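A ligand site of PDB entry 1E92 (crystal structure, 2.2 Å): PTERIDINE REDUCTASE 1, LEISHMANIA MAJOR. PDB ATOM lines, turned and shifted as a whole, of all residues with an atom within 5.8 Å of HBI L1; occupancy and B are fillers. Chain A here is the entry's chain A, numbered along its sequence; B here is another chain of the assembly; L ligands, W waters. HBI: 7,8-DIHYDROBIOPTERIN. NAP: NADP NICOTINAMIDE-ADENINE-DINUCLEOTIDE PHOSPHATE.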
ATOM      1  N   ARG A  17     -29.790  18.872  20.650  1.00  0.00           N
ATOM      2  CA  ARG A  17     -28.347  18.906  20.810  1.00  0.00           C
ATOM      3  C   ARG A  17     -27.593  19.112  19.490  1.00  0.00           C
ATOM      4  O   ARG A  17     -27.932  20.053  18.753  1.00  0.00           O
ATOM      5  CB  ARG A  17     -27.947  17.632  21.570  1.00  0.00           C
ATOM      6  CG  ARG A  17     -28.436  17.705  23.081  1.00  0.00           C
ATOM      7  CD  ARG A  17     -28.432  16.353  23.780  1.00  0.00           C
ATOM      8  NE  ARG A  17     -27.083  15.771  23.782  1.00  0.00           N
ATOM      9  CZ  ARG A  17     -26.108  16.136  24.626  1.00  0.00           C
ATOM     10  NH1 ARG A  17     -26.332  17.080  25.549  1.00  0.00           N
ATOM     11  NH2 ARG A  17     -24.911  15.576  24.533  1.00  0.00           N
ATOM     12  N   ASN A 109     -26.129  11.418  12.206  1.00  0.00           N
ATOM     13  CA  ASN A 109     -25.881  11.935  13.533  1.00  0.00           C
ATOM     14  C   ASN A 109     -26.525  11.106  14.653  1.00  0.00           C
ATOM     15  O   ASN A 109     -25.971  11.044  15.753  1.00  0.00           O
ATOM     16  CB  ASN A 109     -26.391  13.367  13.582  1.00  0.00           C
ATOM     17  CG  ASN A 109     -26.380  13.962  14.960  1.00  0.00           C
ATOM     18  OD1 ASN A 109     -25.360  14.486  15.413  1.00  0.00           O
ATOM     19  ND2 ASN A 109     -27.526  13.903  15.658  1.00  0.00           N
ATOM     20  N   SER A 111     -27.543   8.430  17.320  1.00  0.00           N
ATOM     21  CA  SER A 111     -26.597   7.537  17.984  1.00  0.00           C
ATOM     22  C   SER A 111     -26.929   7.207  19.419  1.00  0.00           C
ATOM     23  O   SER A 111     -27.158   8.126  20.224  1.00  0.00           O
ATOM     24  CB  SER A 111     -25.195   8.205  17.951  1.00  0.00           C
ATOM     25  OG  SER A 111     -24.340   7.779  19.007  1.00  0.00           O
ATOM     26  N   SER A 112     -26.939   5.926  19.761  1.00  0.00           N
ATOM     27  CA  SER A 112     -27.192   5.562  21.156  1.00  0.00           C
ATOM     28  C   SER A 112     -25.823   5.437  21.806  1.00  0.00           C
ATOM     29  O   SER A 112     -24.820   5.091  21.147  1.00  0.00           O
ATOM     30  CB  SER A 112     -28.016   4.265  21.300  1.00  0.00           C
ATOM     31  OG  SER A 112     -27.510   3.184  20.577  1.00  0.00           O
ATOM     32  N   PHE A 113     -25.776   5.743  23.101  1.00  0.00           N
ATOM     33  CA  PHE A 113     -24.492   5.774  23.802  1.00  0.00           C
ATOM     34  C   PHE A 113     -24.716   5.391  25.277  1.00  0.00           C
ATOM     35  O   PHE A 113     -25.310   6.166  26.022  1.00  0.00           O
ATOM     36  CB  PHE A 113     -23.922   7.208  23.670  1.00  0.00           C
ATOM     37  CG  PHE A 113     -22.713   7.528  24.562  1.00  0.00           C
ATOM     38  CD1 PHE A 113     -21.462   6.975  24.302  1.00  0.00           C
ATOM     39  CD2 PHE A 113     -22.851   8.360  25.673  1.00  0.00           C
ATOM     40  CE1 PHE A 113     -20.361   7.250  25.104  1.00  0.00           C
ATOM     41  CE2 PHE A 113     -21.766   8.644  26.500  1.00  0.00           C
ATOM     42  CZ  PHE A 113     -20.520   8.098  26.236  1.00  0.00           C
ATOM     43  N   ASN A 147     -25.330   3.679  15.322  1.00  0.00           N
ATOM     44  CA  ASN A 147     -23.994   4.179  15.045  1.00  0.00           C
ATOM     45  C   ASN A 147     -23.292   3.657  13.789  1.00  0.00           C
ATOM     46  O   ASN A 147     -22.374   4.336  13.281  1.00  0.00           O
ATOM     47  CB  ASN A 147     -23.071   3.888  16.246  1.00  0.00           C
ATOM     48  CG  ASN A 147     -23.408   4.729  17.471  1.00  0.00           C
ATOM     49  OD1 ASN A 147     -23.180   5.933  17.479  1.00  0.00           O
ATOM     50  ND2 ASN A 147     -23.950   4.085  18.513  1.00  0.00           N
ATOM     51  N   ASP A 181     -16.270  10.045  16.544  1.00  0.00           N
ATOM     52  CA  ASP A 181     -15.911  10.432  17.921  1.00  0.00           C
ATOM     53  C   ASP A 181     -14.396  10.607  18.032  1.00  0.00           C
ATOM     54  O   ASP A 181     -13.646   9.659  17.866  1.00  0.00           O
ATOM     55  CB  ASP A 181     -16.401   9.327  18.890  1.00  0.00           C
ATOM     56  CG  ASP A 181     -16.144   9.661  20.364  1.00  0.00           C
ATOM     57  OD1 ASP A 181     -15.291  10.540  20.677  1.00  0.00           O
ATOM     58  OD2 ASP A 181     -16.798   9.019  21.215  1.00  0.00           O
ATOM     59  N   LEU A 188     -13.283   5.019  26.242  1.00  0.00           N
ATOM     60  CA  LEU A 188     -13.988   5.355  27.450  1.00  0.00           C
ATOM     61  C   LEU A 188     -14.197   3.976  28.102  1.00  0.00           C
ATOM     62  O   LEU A 188     -14.719   3.042  27.464  1.00  0.00           O
ATOM     63  CB  LEU A 188     -15.292   6.003  27.052  1.00  0.00           C
ATOM     64  CG  LEU A 188     -16.042   6.799  28.108  1.00  0.00           C
ATOM     65  CD1 LEU A 188     -15.125   7.877  28.744  1.00  0.00           C
ATOM     66  CD2 LEU A 188     -17.264   7.397  27.428  1.00  0.00           C
ATOM     67  N   TYR A 194     -20.216   0.556  21.832  1.00  0.00           N
ATOM     68  CA  TYR A 194     -20.304   1.889  21.275  1.00  0.00           C
ATOM     69  C   TYR A 194     -18.964   2.257  20.573  1.00  0.00           C
ATOM     70  O   TYR A 194     -18.960   2.805  19.463  1.00  0.00           O
ATOM     71  CB  TYR A 194     -20.572   2.907  22.405  1.00  0.00           C
ATOM     72  CG  TYR A 194     -20.231   4.326  21.962  1.00  0.00           C
ATOM     73  CD1 TYR A 194     -21.151   5.098  21.234  1.00  0.00           C
ATOM     74  CD2 TYR A 194     -18.975   4.874  22.255  1.00  0.00           C
ATOM     75  CE1 TYR A 194     -20.823   6.393  20.811  1.00  0.00           C
ATOM     76  CE2 TYR A 194     -18.629   6.157  21.821  1.00  0.00           C
ATOM     77  CZ  TYR A 194     -19.552   6.897  21.111  1.00  0.00           C
ATOM     78  OH  TYR A 194     -19.208   8.169  20.719  1.00  0.00           O
ATOM     79  N   LYS A 198     -18.441   3.033  16.527  1.00  0.00           N
ATOM     80  CA  LYS A 198     -17.836   4.230  15.957  1.00  0.00           C
ATOM     81  C   LYS A 198     -16.641   3.852  15.051  1.00  0.00           C
ATOM     82  O   LYS A 198     -16.358   4.515  14.040  1.00  0.00           O
ATOM     83  CB  LYS A 198     -17.404   5.213  17.066  1.00  0.00           C
ATOM     84  CG  LYS A 198     -18.577   5.970  17.732  1.00  0.00           C
ATOM     85  CD  LYS A 198     -19.493   6.718  16.696  1.00  0.00           C
ATOM     86  CE  LYS A 198     -20.399   7.718  17.431  1.00  0.00           C
ATOM     87  NZ  LYS A 198     -21.446   8.278  16.549  1.00  0.00           N
ATOM     88  N   GLY A 225     -15.211  15.904  20.618  1.00  0.00           N
ATOM     89  CA  GLY A 225     -14.497  15.414  21.790  1.00  0.00           C
ATOM     90  C   GLY A 225     -15.574  15.388  22.872  1.00  0.00           C
ATOM     91  O   GLY A 225     -16.269  14.397  23.066  1.00  0.00           O
ATOM     92  N   LEU A 226     -15.728  16.494  23.590  1.00  0.00           N
ATOM     93  CA  LEU A 226     -16.782  16.645  24.599  1.00  0.00           C
ATOM     94  C   LEU A 226     -17.624  17.824  24.111  1.00  0.00           C
ATOM     95  O   LEU A 226     -17.067  18.923  23.956  1.00  0.00           O
ATOM     96  CB  LEU A 226     -16.187  16.995  25.961  1.00  0.00           C
ATOM     97  CG  LEU A 226     -15.186  15.984  26.518  1.00  0.00           C
ATOM     98  CD1 LEU A 226     -14.693  16.426  27.938  1.00  0.00           C
ATOM     99  CD2 LEU A 226     -15.840  14.602  26.607  1.00  0.00           C
ATOM    100  N   SER A 227     -18.928  17.637  23.855  1.00  0.00           N
ATOM    101  CA  SER A 227     -19.810  18.736  23.413  1.00  0.00           C
ATOM    102  C   SER A 227     -21.098  18.740  24.187  1.00  0.00           C
ATOM    103  O   SER A 227     -21.696  17.670  24.361  1.00  0.00           O
ATOM    104  CB  SER A 227     -20.165  18.630  21.945  1.00  0.00           C
ATOM    105  OG  SER A 227     -18.976  18.487  21.210  1.00  0.00           O
ATOM    106  N   LEU A 229     -21.696  18.689  27.104  1.00  0.00           N
ATOM    107  CA  LEU A 229     -21.567  17.579  28.033  1.00  0.00           C
ATOM    108  C   LEU A 229     -22.765  17.447  28.998  1.00  0.00           C
ATOM    109  O   LEU A 229     -23.111  18.385  29.674  1.00  0.00           O
ATOM    110  CB  LEU A 229     -20.282  17.771  28.844  1.00  0.00           C
ATOM    111  CG  LEU A 229     -19.790  16.651  29.768  1.00  0.00           C
ATOM    112  CD1 LEU A 229     -19.396  15.416  28.934  1.00  0.00           C
ATOM    113  CD2 LEU A 229     -18.599  17.154  30.559  1.00  0.00           C
ATOM    114  N   VAL A 230     -23.410  16.283  29.022  1.00  0.00           N
ATOM    115  CA  VAL A 230     -24.550  16.074  29.929  1.00  0.00           C
ATOM    116  C   VAL A 230     -24.031  16.345  31.350  1.00  0.00           C
ATOM    117  O   VAL A 230     -22.980  15.848  31.740  1.00  0.00           O
ATOM    118  CB  VAL A 230     -25.049  14.618  29.880  1.00  0.00           C
ATOM    119  CG1 VAL A 230     -26.278  14.488  30.763  1.00  0.00           C
ATOM    120  CG2 VAL A 230     -25.362  14.226  28.436  1.00  0.00           C
ATOM    121  N   ARG B 287      -6.468   8.997  28.518  1.00  0.00           N
ATOM    122  CA  ARG B 287      -6.800  10.391  28.235  1.00  0.00           C
ATOM    123  C   ARG B 287      -6.722  11.102  29.589  1.00  0.00           C
ATOM    124  O   ARG B 287      -6.736  10.470  30.639  1.00  0.00           O
ATOM    125  CB  ARG B 287      -8.230  10.489  27.642  1.00  0.00           C
ATOM    126  CG  ARG B 287      -9.319   9.839  28.501  1.00  0.00           C
ATOM    127  CD  ARG B 287     -10.729  10.137  27.976  1.00  0.00           C
ATOM    128  NE  ARG B 287     -11.160   9.283  26.864  1.00  0.00           N
ATOM    129  CZ  ARG B 287     -12.374   9.345  26.309  1.00  0.00           C
ATOM    130  NH1 ARG B 287     -13.261  10.261  26.740  1.00  0.00           N
ATOM    131  NH2 ARG B 287     -12.732   8.473  25.385  1.00  0.00           N
HETATM  132  N1  HBI L   1     -22.494   9.850  21.863  1.00  0.00           N
HETATM  133  N2  HBI L   1     -24.700   9.621  21.159  1.00  0.00           N
HETATM  134  C2  HBI L   1     -23.770  10.210  22.049  1.00  0.00           C
HETATM  135  N3  HBI L   1     -24.229  11.056  22.984  1.00  0.00           N
HETATM  136  C4  HBI L   1     -23.346  11.620  23.827  1.00  0.00           C
HETATM  137  O4  HBI L   1     -23.814  12.482  24.773  1.00  0.00           O
HETATM  138  C4A HBI L   1     -21.920  11.318  23.748  1.00  0.00           C
HETATM  139  C8A HBI L   1     -21.555  10.378  22.685  1.00  0.00           C
HETATM  140  N8  HBI L   1     -20.151  10.001  22.475  1.00  0.00           N
HETATM  141  C7  HBI L   1     -19.147  10.458  23.537  1.00  0.00           C
HETATM  142  C6  HBI L   1     -19.630  11.557  24.555  1.00  0.00           C
HETATM  143  N5  HBI L   1     -20.917  11.882  24.614  1.00  0.00           N
HETATM  144  C9  HBI L   1     -18.636  12.217  25.494  1.00  0.00           C
HETATM  145  O9  HBI L   1     -19.026  13.629  25.687  1.00  0.00           O
HETATM  146  C10 HBI L   1     -18.488  11.428  26.864  1.00  0.00           C
HETATM  147  O10 HBI L   1     -17.168  11.618  27.494  1.00  0.00           O
HETATM  148  C11 HBI L   1     -19.617  11.830  27.907  1.00  0.00           C
HETATM  149  PA  NAP L   2     -27.359  12.348  21.542  1.00  0.00           P
HETATM  150  O1A NAP L   2     -26.810  11.368  22.521  1.00  0.00           O
HETATM  151  O2A NAP L   2     -28.008  13.517  22.063  1.00  0.00           O
HETATM  152  O5B NAP L   2     -28.305  11.548  20.531  1.00  0.00           O
HETATM  153  C5B NAP L   2     -28.659  12.000  19.250  1.00  0.00           C
HETATM  154  C4B NAP L   2     -29.977  11.384  18.798  1.00  0.00           C
HETATM  155  O4B NAP L   2     -29.750  10.046  18.347  1.00  0.00           O
HETATM  156  C3B NAP L   2     -30.980  11.250  19.954  1.00  0.00           C
HETATM  157  O3B NAP L   2     -31.713  12.480  20.056  1.00  0.00           O
HETATM  158  C2B NAP L   2     -31.875  10.096  19.442  1.00  0.00           C
HETATM  159  O2B NAP L   2     -33.141  10.593  18.893  1.00  0.00           O
HETATM  160  C1B NAP L   2     -31.034   9.375  18.345  1.00  0.00           C
HETATM  161  N9A NAP L   2     -31.010   7.952  18.552  1.00  0.00           N
HETATM  162  C8A NAP L   2     -30.381   7.219  19.530  1.00  0.00           C
HETATM  163  N7A NAP L   2     -30.641   5.895  19.343  1.00  0.00           N
HETATM  164  C5A NAP L   2     -31.406   5.844  18.270  1.00  0.00           C
HETATM  165  C6A NAP L   2     -31.960   4.722  17.662  1.00  0.00           C
HETATM  166  N6A NAP L   2     -31.763   3.466  18.110  1.00  0.00           N
HETATM  167  N1A NAP L   2     -32.744   4.900  16.545  1.00  0.00           N
HETATM  168  C2A NAP L   2     -32.973   6.145  16.057  1.00  0.00           C
HETATM  169  N3A NAP L   2     -32.443   7.226  16.635  1.00  0.00           N
HETATM  170  C4A NAP L   2     -31.642   7.098  17.763  1.00  0.00           C
HETATM  171  O3  NAP L   2     -26.163  12.856  20.595  1.00  0.00           O
HETATM  172  PN  NAP L   2     -25.204  14.165  20.604  1.00  0.00           P
HETATM  173  O1N NAP L   2     -24.636  14.297  21.954  1.00  0.00           O
HETATM  174  O2N NAP L   2     -25.992  15.332  20.091  1.00  0.00           O
HETATM  175  O5D NAP L   2     -24.084  13.777  19.550  1.00  0.00           O
HETATM  176  C5D NAP L   2     -24.350  13.816  18.131  1.00  0.00           C
HETATM  177  C4D NAP L   2     -23.343  12.901  17.412  1.00  0.00           C
HETATM  178  O4D NAP L   2     -22.008  13.300  17.816  1.00  0.00           O
HETATM  179  C3D NAP L   2     -23.503  11.414  17.794  1.00  0.00           C
HETATM  180  O3D NAP L   2     -23.213  10.567  16.677  1.00  0.00           O
HETATM  181  C2D NAP L   2     -22.436  11.220  18.898  1.00  0.00           C
HETATM  182  O2D NAP L   2     -21.989   9.854  19.042  1.00  0.00           O
HETATM  183  C1D NAP L   2     -21.344  12.154  18.448  1.00  0.00           C
HETATM  184  N1N NAP L   2     -20.492  12.557  19.556  1.00  0.00           N
HETATM  185  C2N NAP L   2     -21.049  13.438  20.585  1.00  0.00           C
HETATM  186  C3N NAP L   2     -20.211  13.818  21.642  1.00  0.00           C
HETATM  187  C7N NAP L   2     -20.675  14.754  22.786  1.00  0.00           C
HETATM  188  O7N NAP L   2     -19.846  15.171  23.567  1.00  0.00           O
HETATM  189  N7N NAP L   2     -21.990  15.047  22.831  1.00  0.00           N
HETATM  190  C4N NAP L   2     -18.877  13.338  21.675  1.00  0.00           C
HETATM  191  C5N NAP L   2     -18.327  12.472  20.672  1.00  0.00           C
HETATM  192  C6N NAP L   2     -19.150  12.085  19.611  1.00  0.00           C
HETATM  193  P2B NAP L   2     -34.539  10.756  19.708  1.00  0.00           P
HETATM  194  O1X NAP L   2     -35.471  11.365  18.713  1.00  0.00           O
HETATM  195  O2X NAP L   2     -34.940   9.414  20.172  1.00  0.00           O
HETATM  196  O3X NAP L   2     -34.207  11.764  20.808  1.00  0.00           O
HETATM  197  O   HOH W   1     -22.314  14.351  26.711  1.00  0.00           O
HETATM  198  O   HOH W   2     -15.681  10.411  25.474  1.00  0.00           O
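O7N of NAP L2 lies within hydrogen-bond range of N of Ser 227 (2.6 Å). OG of Ser 111 sits at hydrogen-bond distance from N2 of HBI L1, at 2.9 Å. O of Asn 109 sits at hydrogen-bond distance from O3D of NAP L2 (2.9 Å). The side-chain hydroxyl (OH) of Tyr 194 sits at hydrogen-bond distance from a nitrogen (N8) of HBI L1. The backbone NH of Ser 111 is in hydrogen-bond range of an oxygen (O4B) of NAP L2 (2.9 Å). O of Ser 227 lies within hydrogen-bond range of N7N of NAP L2. NH2 of Arg 17 lies within salt-bridge range of O1N of NAP L2 (2.9 Å). The side-chain hydroxyl of Ser 111 sits at hydrogen-bond distance from an oxygen (O2D) of NAP L2. The backbone carbonyl oxygen (O) of Ser 111 is in hydrogen-bond range of a nitrogen (N2) of HBI L1 (3.0 Å). The guanidinium group (NH2) of Arg 17 sits at hydrogen-bond distance from an oxygen (O4) of HBI L1 (3.3 Å). An oxygen (O3D) of NAP L2 lies within hydrogen-bond range of the side-chain amino group (NZ) of Lys 198 (2.9 Å).
N3 of HBI L1 lies within hydrogen-bond range of O1A of NAP L2 (2.6 Å).
The side-chain hydroxyl (OH) of Tyr 194 is in hydrogen-bond range of the side-chain carboxylate (OD2) of Asp 181. The side-chain hydroxyl of Ser 111 is in hydrogen-bond range of the side-chain amide oxygen of Asn 147, at 2.7 Å.
Phe 113 touches HBI L1. Asp 181 touches HBI L1. Gly 225 touches HBI L1 (O to O9, 3.9 Å). CD2 of Leu 226 touches O10 of HBI L1, 3.4 Å away. CD1 of Leu 229 touches O9 of HBI L1, at 3.7 Å. Hydrophobic or aromatic side chains within 4 Å of HBI L1: Phe 113, Tyr 194, Leu 226 and Leu 229. Eight residues have an atom within 4 Å of HBI L1: Arg 17, Ser 111, Phe 113, Asp 181, Tyr 194, Gly 225, Leu 226 and Leu 229. The nearest printed residue that does not touch HBI L1 is Arg 287 of chain B (4.2 Å).
Water W2 lies within hydrogen-bond range of the guanidinium group (NH1) of Arg 287 of chain B and an oxygen (O10) of HBI L1. Water W1 bridges an oxygen (O4) of HBI L1 (3.1 Å) and the backbone NH of Val 230 (3.2 Å).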
